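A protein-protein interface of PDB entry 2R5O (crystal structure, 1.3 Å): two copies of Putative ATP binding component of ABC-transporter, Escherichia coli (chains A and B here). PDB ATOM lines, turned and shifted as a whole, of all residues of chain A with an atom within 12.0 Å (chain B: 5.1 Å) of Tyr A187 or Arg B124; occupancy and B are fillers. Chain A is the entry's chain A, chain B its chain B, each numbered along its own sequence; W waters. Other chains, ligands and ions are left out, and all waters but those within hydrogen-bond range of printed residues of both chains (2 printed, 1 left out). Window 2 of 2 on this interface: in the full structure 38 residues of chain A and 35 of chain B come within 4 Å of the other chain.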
ATOM      1  N   SER A 182     -12.947  16.609  10.666  1.00  0.00           N
ATOM      2  CA  SER A 182     -13.109  17.975  10.214  1.00  0.00           C
ATOM      3  C   SER A 182     -13.932  18.790  11.192  1.00  0.00           C
ATOM      4  O   SER A 182     -14.916  18.297  11.772  1.00  0.00           O
ATOM      5  CB  SER A 182     -13.832  17.980   8.879  1.00  0.00           C
ATOM      6  OG  SER A 182     -13.889  19.289   8.300  1.00  0.00           O
ATOM      7  N   SER A 183     -13.566  20.067  11.331  1.00  0.00           N
ATOM      8  CA  SER A 183     -14.437  21.070  11.933  1.00  0.00           C
ATOM      9  C   SER A 183     -15.220  21.766  10.830  1.00  0.00           C
ATOM     10  O   SER A 183     -14.937  21.587   9.641  1.00  0.00           O
ATOM     11  CB  SER A 183     -13.666  22.058  12.805  1.00  0.00           C
ATOM     12  OG  SER A 183     -12.768  22.807  12.040  1.00  0.00           O
ATOM     13  N   PHE A 184     -16.194  22.579  11.210  1.00  0.00           N
ATOM     14  CA  PHE A 184     -17.087  23.198  10.254  1.00  0.00           C
ATOM     15  C   PHE A 184     -17.469  24.587  10.721  1.00  0.00           C
ATOM     16  O   PHE A 184     -17.784  24.767  11.892  1.00  0.00           O
ATOM     17  CB  PHE A 184     -18.357  22.378  10.086  1.00  0.00           C
ATOM     18  CG  PHE A 184     -19.356  23.038   9.210  1.00  0.00           C
ATOM     19  CD1 PHE A 184     -19.218  22.965   7.818  1.00  0.00           C
ATOM     20  CD2 PHE A 184     -20.384  23.811   9.738  1.00  0.00           C
ATOM     21  CE1 PHE A 184     -20.095  23.593   7.002  1.00  0.00           C
ATOM     22  CE2 PHE A 184     -21.273  24.449   8.897  1.00  0.00           C
ATOM     23  CZ  PHE A 184     -21.114  24.338   7.532  1.00  0.00           C
ATOM     24  N   THR A 185     -17.497  25.541   9.815  1.00  0.00           N
ATOM     25  CA  THR A 185     -18.067  26.856  10.086  1.00  0.00           C
ATOM     26  C   THR A 185     -18.715  27.395   8.832  1.00  0.00           C
ATOM     27  O   THR A 185     -18.376  26.994   7.731  1.00  0.00           O
ATOM     28  CB  THR A 185     -16.962  27.892  10.452  1.00  0.00           C
ATOM     29  OG1 THR A 185     -15.834  27.207  11.023  1.00  0.00           O
ATOM     30  CG2 THR A 185     -17.503  28.967  11.385  1.00  0.00           C
ATOM     31  N   SER A 186     -19.640  28.331   8.991  1.00  0.00           N
ATOM     32  CA  SER A 186     -20.273  28.959   7.825  1.00  0.00           C
ATOM     33  C   SER A 186     -20.254  30.469   7.942  1.00  0.00           C
ATOM     34  O   SER A 186     -20.263  31.002   9.060  1.00  0.00           O
ATOM     35  CB  SER A 186     -21.696  28.456   7.647  1.00  0.00           C
ATOM     36  OG  SER A 186     -22.485  28.758   8.764  1.00  0.00           O
ATOM     37  N   TYR A 187     -20.275  31.144   6.790  1.00  0.00           N
ATOM     38  CA  TYR A 187     -20.129  32.564   6.677  1.00  0.00           C
ATOM     39  C   TYR A 187     -21.268  33.097   5.828  1.00  0.00           C
ATOM     40  O   TYR A 187     -21.638  32.482   4.817  1.00  0.00           O
ATOM     41  CB  TYR A 187     -18.787  32.863   6.011  1.00  0.00           C
ATOM     42  CG  TYR A 187     -17.602  32.229   6.722  1.00  0.00           C
ATOM     43  CD1 TYR A 187     -17.122  30.964   6.365  1.00  0.00           C
ATOM     44  CD2 TYR A 187     -16.948  32.910   7.739  1.00  0.00           C
ATOM     45  CE1 TYR A 187     -16.022  30.414   7.019  1.00  0.00           C
ATOM     46  CE2 TYR A 187     -15.854  32.350   8.399  1.00  0.00           C
ATOM     47  CZ  TYR A 187     -15.404  31.121   8.038  1.00  0.00           C
ATOM     48  OH  TYR A 187     -14.321  30.608   8.700  1.00  0.00           O
ATOM     49  N   LEU B  23     -18.755  37.262  -1.714  1.00  0.00           N
ATOM     50  CA  LEU B  23     -20.177  36.937  -1.544  1.00  0.00           C
ATOM     51  C   LEU B  23     -21.069  37.707  -2.506  1.00  0.00           C
ATOM     52  O   LEU B  23     -22.215  37.316  -2.728  1.00  0.00           O
ATOM     53  CB  LEU B  23     -20.653  37.205  -0.109  1.00  0.00           C
ATOM     54  CG  LEU B  23     -20.124  36.329   1.030  1.00  0.00           C
ATOM     55  CD1 LEU B  23     -20.870  36.660   2.315  1.00  0.00           C
ATOM     56  CD2 LEU B  23     -20.243  34.845   0.717  1.00  0.00           C
ATOM     57  N   LEU B  75     -13.086  25.468   1.394  1.00  0.00           N
ATOM     58  CA  LEU B  75     -14.214  26.393   1.374  1.00  0.00           C
ATOM     59  C   LEU B  75     -15.003  26.222   0.093  1.00  0.00           C
ATOM     60  O   LEU B  75     -14.433  26.086  -0.983  1.00  0.00           O
ATOM     61  CB  LEU B  75     -13.744  27.852   1.473  1.00  0.00           C
ATOM     62  CG  LEU B  75     -12.960  28.185   2.759  1.00  0.00           C
ATOM     63  CD1 LEU B  75     -11.482  28.075   2.592  1.00  0.00           C
ATOM     64  CD2 LEU B  75     -13.323  29.537   3.282  1.00  0.00           C
ATOM     65  N   MET B  76     -16.331  26.261   0.218  1.00  0.00           N
ATOM     66  CA  MET B  76     -17.229  26.219  -0.931  1.00  0.00           C
ATOM     67  C   MET B  76     -18.205  27.370  -0.839  1.00  0.00           C
ATOM     68  O   MET B  76     -18.728  27.643   0.243  1.00  0.00           O
ATOM     69  CB  MET B  76     -17.952  24.853  -1.021  1.00  0.00           C
ATOM     70  CG  MET B  76     -18.611  24.436   0.296  1.00  0.00           C
ATOM     71  SD  MET B  76     -19.533  22.845   0.252  1.00  0.00           S
ATOM     72  CE  MET B  76     -20.986  23.435  -0.541  1.00  0.00           C
ATOM     73  N   LYS B  77     -18.500  27.991  -1.966  1.00  0.00           N
ATOM     74  CA  LYS B  77     -19.447  29.083  -2.037  1.00  0.00           C
ATOM     75  C   LYS B  77     -20.686  28.639  -2.792  1.00  0.00           C
ATOM     76  O   LYS B  77     -20.587  28.044  -3.878  1.00  0.00           O
ATOM     77  CB  LYS B  77     -18.820  30.271  -2.760  1.00  0.00           C
ATOM     78  CG  LYS B  77     -19.715  31.517  -2.797  1.00  0.00           C
ATOM     79  CD  LYS B  77     -19.017  32.736  -3.397  1.00  0.00           C
ATOM     80  CE  LYS B  77     -18.976  32.730  -4.893  1.00  0.00           C
ATOM     81  NZ  LYS B  77     -18.645  34.094  -5.419  1.00  0.00           N
ATOM     82  N   VAL B  78     -21.849  28.951  -2.217  1.00  0.00           N
ATOM     83  CA  VAL B  78     -23.134  28.517  -2.758  1.00  0.00           C
ATOM     84  C   VAL B  78     -24.075  29.699  -2.882  1.00  0.00           C
ATOM     85  O   VAL B  78     -24.182  30.500  -1.967  1.00  0.00           O
ATOM     86  CB  VAL B  78     -23.789  27.442  -1.849  1.00  0.00           C
ATOM     87  CG1 VAL B  78     -25.053  26.905  -2.451  1.00  0.00           C
ATOM     88  CG2 VAL B  78     -22.806  26.302  -1.575  1.00  0.00           C
ATOM     89  N   PHE B  80     -28.150  30.364  -3.280  1.00  0.00           N
ATOM     90  CA  PHE B  80     -29.440  29.705  -3.077  1.00  0.00           C
ATOM     91  C   PHE B  80     -30.531  30.441  -3.815  1.00  0.00           C
ATOM     92  O   PHE B  80     -30.612  31.663  -3.745  1.00  0.00           O
ATOM     93  CB  PHE B  80     -29.743  29.648  -1.581  1.00  0.00           C
ATOM     94  CG  PHE B  80     -28.774  28.789  -0.830  1.00  0.00           C
ATOM     95  CD1 PHE B  80     -28.972  27.425  -0.684  1.00  0.00           C
ATOM     96  CD2 PHE B  80     -27.622  29.340  -0.301  1.00  0.00           C
ATOM     97  CE1 PHE B  80     -28.051  26.644  -0.009  1.00  0.00           C
ATOM     98  CE2 PHE B  80     -26.699  28.547   0.361  1.00  0.00           C
ATOM     99  CZ  PHE B  80     -26.928  27.189   0.488  1.00  0.00           C
ATOM    100  N   ILE B 116     -28.822  25.392   9.549  1.00  0.00           N
ATOM    101  CA  ILE B 116     -28.419  26.556   8.760  1.00  0.00           C
ATOM    102  C   ILE B 116     -29.587  26.886   7.856  1.00  0.00           C
ATOM    103  O   ILE B 116     -29.978  26.054   7.041  1.00  0.00           O
ATOM    104  CB  ILE B 116     -27.166  26.257   7.887  1.00  0.00           C
ATOM    105  CG1 ILE B 116     -25.994  25.818   8.763  1.00  0.00           C
ATOM    106  CG2 ILE B 116     -26.816  27.471   7.042  1.00  0.00           C
ATOM    107  CD1 ILE B 116     -24.850  25.187   7.965  1.00  0.00           C
ATOM    108  N   SER B 117     -30.168  28.067   7.995  1.00  0.00           N
ATOM    109  CA  SER B 117     -31.276  28.510   7.145  1.00  0.00           C
ATOM    110  C   SER B 117     -30.781  29.561   6.146  1.00  0.00           C
ATOM    111  O   SER B 117     -29.823  30.297   6.403  1.00  0.00           O
ATOM    112  CB  SER B 117     -32.415  29.114   7.982  1.00  0.00           C
ATOM    113  OG  SER B 117     -32.867  28.248   9.006  1.00  0.00           O
ATOM    114  N   VAL B 118     -31.445  29.634   5.006  1.00  0.00           N
ATOM    115  CA  VAL B 118     -31.098  30.615   3.992  1.00  0.00           C
ATOM    116  C   VAL B 118     -32.358  31.193   3.381  1.00  0.00           C
ATOM    117  O   VAL B 118     -33.432  30.585   3.419  1.00  0.00           O
ATOM    118  CB  VAL B 118     -30.231  30.016   2.833  1.00  0.00           C
ATOM    119  CG1 VAL B 118     -28.960  29.384   3.369  1.00  0.00           C
ATOM    120  CG2 VAL B 118     -31.021  29.007   1.991  1.00  0.00           C
ATOM    121  N   SER B 119     -32.194  32.381   2.812  1.00  0.00           N
ATOM    122  CA  SER B 119     -33.220  33.048   2.041  1.00  0.00           C
ATOM    123  C   SER B 119     -32.852  33.063   0.575  1.00  0.00           C
ATOM    124  O   SER B 119     -31.680  33.043   0.208  1.00  0.00           O
ATOM    125  CB  SER B 119     -33.406  34.485   2.519  1.00  0.00           C
ATOM    126  OG  SER B 119     -33.799  34.519   3.876  1.00  0.00           O
ATOM    127  N   ASP B 122     -29.526  34.311  -1.266  1.00  0.00           N
ATOM    128  CA  ASP B 122     -28.372  34.342  -0.372  1.00  0.00           C
ATOM    129  C   ASP B 122     -27.165  33.623  -0.986  1.00  0.00           C
ATOM    130  O   ASP B 122     -27.311  32.613  -1.659  1.00  0.00           O
ATOM    131  CB  ASP B 122     -28.667  33.646   0.961  1.00  0.00           C
ATOM    132  CG  ASP B 122     -29.496  34.475   1.920  1.00  0.00           C
ATOM    133  OD1 ASP B 122     -29.786  35.646   1.617  1.00  0.00           O
ATOM    134  OD2 ASP B 122     -29.875  33.904   2.982  1.00  0.00           O
ATOM    135  N   VAL B 123     -25.990  34.176  -0.731  1.00  0.00           N
ATOM    136  CA  VAL B 123     -24.707  33.579  -1.086  1.00  0.00           C
ATOM    137  C   VAL B 123     -23.990  33.306   0.217  1.00  0.00           C
ATOM    138  O   VAL B 123     -23.858  34.202   1.055  1.00  0.00           O
ATOM    139  CB  VAL B 123     -23.869  34.512  -1.995  1.00  0.00           C
ATOM    140  CG1 VAL B 123     -22.548  33.864  -2.349  1.00  0.00           C
ATOM    141  CG2 VAL B 123     -24.622  34.880  -3.252  1.00  0.00           C
ATOM    142  N   ARG B 124     -23.563  32.064   0.406  1.00  0.00           N
ATOM    143  CA  ARG B 124     -22.918  31.636   1.646  1.00  0.00           C
ATOM    144  C   ARG B 124     -21.622  30.911   1.341  1.00  0.00           C
ATOM    145  O   ARG B 124     -21.518  30.250   0.316  1.00  0.00           O
ATOM    146  CB  ARG B 124     -23.842  30.677   2.401  1.00  0.00           C
ATOM    147  CG  ARG B 124     -25.194  31.233   2.794  1.00  0.00           C
ATOM    148  CD  ARG B 124     -25.117  32.255   3.892  1.00  0.00           C
ATOM    149  NE  ARG B 124     -26.458  32.757   4.192  1.00  0.00           N
ATOM    150  CZ  ARG B 124     -27.274  32.247   5.112  1.00  0.00           C
ATOM    151  NH1 ARG B 124     -26.920  31.204   5.871  1.00  0.00           N
ATOM    152  NH2 ARG B 124     -28.464  32.790   5.265  1.00  0.00           N
ATOM    153  N   VAL B 125     -20.683  30.998   2.269  1.00  0.00           N
ATOM    154  CA  VAL B 125     -19.462  30.224   2.217  1.00  0.00           C
ATOM    155  C   VAL B 125     -19.426  29.261   3.395  1.00  0.00           C
ATOM    156  O   VAL B 125     -19.696  29.636   4.541  1.00  0.00           O
ATOM    157  CB  VAL B 125     -18.211  31.123   2.216  1.00  0.00           C
ATOM    158  CG1 VAL B 125     -16.913  30.315   2.376  1.00  0.00           C
ATOM    159  CG2 VAL B 125     -18.175  31.945   0.956  1.00  0.00           C
ATOM    160  N   PHE B 126     -19.101  28.010   3.109  1.00  0.00           N
ATOM    161  CA  PHE B 126     -19.014  26.941   4.094  1.00  0.00           C
ATOM    162  C   PHE B 126     -17.584  26.451   4.132  1.00  0.00           C
ATOM    163  O   PHE B 126     -16.982  26.231   3.083  1.00  0.00           O
ATOM    164  CB  PHE B 126     -19.971  25.810   3.714  1.00  0.00           C
ATOM    165  CG  PHE B 126     -21.380  26.274   3.545  1.00  0.00           C
ATOM    166  CD1 PHE B 126     -22.101  26.698   4.647  1.00  0.00           C
ATOM    167  CD2 PHE B 126     -21.968  26.318   2.317  1.00  0.00           C
ATOM    168  CE1 PHE B 126     -23.408  27.155   4.508  1.00  0.00           C
ATOM    169  CE2 PHE B 126     -23.295  26.753   2.168  1.00  0.00           C
ATOM    170  CZ  PHE B 126     -24.015  27.161   3.270  1.00  0.00           C
ATOM    171  N   LYS B 127     -17.055  26.269   5.332  1.00  0.00           N
ATOM    172  CA  LYS B 127     -15.646  25.964   5.528  1.00  0.00           C
ATOM    173  C   LYS B 127     -15.489  24.705   6.346  1.00  0.00           C
ATOM    174  O   LYS B 127     -15.957  24.646   7.499  1.00  0.00           O
ATOM    175  CB  LYS B 127     -14.966  27.118   6.247  1.00  0.00           C
ATOM    176  CG  LYS B 127     -13.477  26.874   6.476  1.00  0.00           C
ATOM    177  CD  LYS B 127     -12.842  27.813   7.496  1.00  0.00           C
ATOM    178  CE  LYS B 127     -12.477  29.156   6.952  1.00  0.00           C
ATOM    179  NZ  LYS B 127     -11.744  29.965   8.031  1.00  0.00           N
HETATM  180  O   HOH W   1     -24.334  30.556   7.106  1.00  0.00           O
HETATM  181  O   HOH W   2     -14.072  25.177   9.712  1.00  0.00           O
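The backbone NH of Val B78 is in hydrogen-bond range of the backbone carbonyl oxygen of Arg B124, 2.9 Å away. The guanidinium group of Arg B124 sits at hydrogen-bond distance from the backbone carbonyl oxygen of Ser B117 (3.1 Å). OD2 of Asp B122 lies within salt-bridge range of NH2 of Arg B124. The backbone NH (N) of Phe B126 is in hydrogen-bond range of the backbone carbonyl oxygen (O) of Met B76, 2.9 Å away.
Hydrophobic or aromatic side chains of chain A within 4 Å of the printed part of chain B: Phe A184 and Tyr A187. Of the 16 printed residues of chain B, 5 touch a printed residue of chain A.
No position is printed for both chains.
Among the printed residues, pairs that only touch across the chains: Ser A183 with Lys B127 (3.9 Å), Phe A184 with Ile B116 (3.8 Å), Phe A184 with Phe B126 (3.9 Å), Phe A184 with Lys B127 (3.3 Å), Thr A185 with Phe B126 (3.7 Å), Ser A186 with Val B125 (3.4 Å), Ser A186 with Phe B126 (3.5 Å) and Tyr A187 with Arg B124 (3.5 Å).
Water W1 lies within hydrogen-bond range of NH1 of Arg B124 and OG of Ser A186. Water W2 bridges O of Lys B127 (3.0 Å) and OG1 of Thr A185 (3.0 Å).
The side-chain amino group (NZ) of Lys B127 lies within hydrogen-bond range of the side-chain hydroxyl (OH) of Tyr A187 (2.7 Å). The backbone carbonyl oxygen of Thr A185 sits at hydrogen-bond distance from the backbone NH of Lys B127 (2.8 Å). The backbone NH (N) of Tyr A187 lies within hydrogen-bond range of the backbone carbonyl oxygen (O) of Val B125 (2.8 Å).
Printed residues of chain B within 4 Å of Tyr A187: Arg B124, Val B125 and Lys B127. Of the printed residues of chain A, Arg B124 touches Tyr A187 (3.5 Å). No residue of chain A comes within 4 Å of Leu B23. No residue of chain A comes within 4 Å of Lys B77. Val B78 touches none of the printed residues of chain A. Ile B116 touches just one residue of chain A: Phe A184. No residue of chain A comes within 4 Å of Ser B119. No residue of chain A comes within 4 Å of Asp B122. No residue of chain A comes within 4 Å of Val B123. Printed residues of chain B within 4 Å of Ser A186: Val B125 and Phe B126. Of the printed residues of chain B, Ser A183 touches Lys B127. Of the printed residues of chain B, Thr A185 touches Phe B126 and Lys B127. Of the printed residues of chain A, Val B125 touches Ser A186 (3.4 Å) and Tyr A187 (2.8 Å). Ser B117 touches none of the printed residues of chain A. Phe B80 touches none of the printed residues of chain A. The nearest printed residue of chain B that does not touch Tyr A187 is Leu B75 (4.7 Å).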
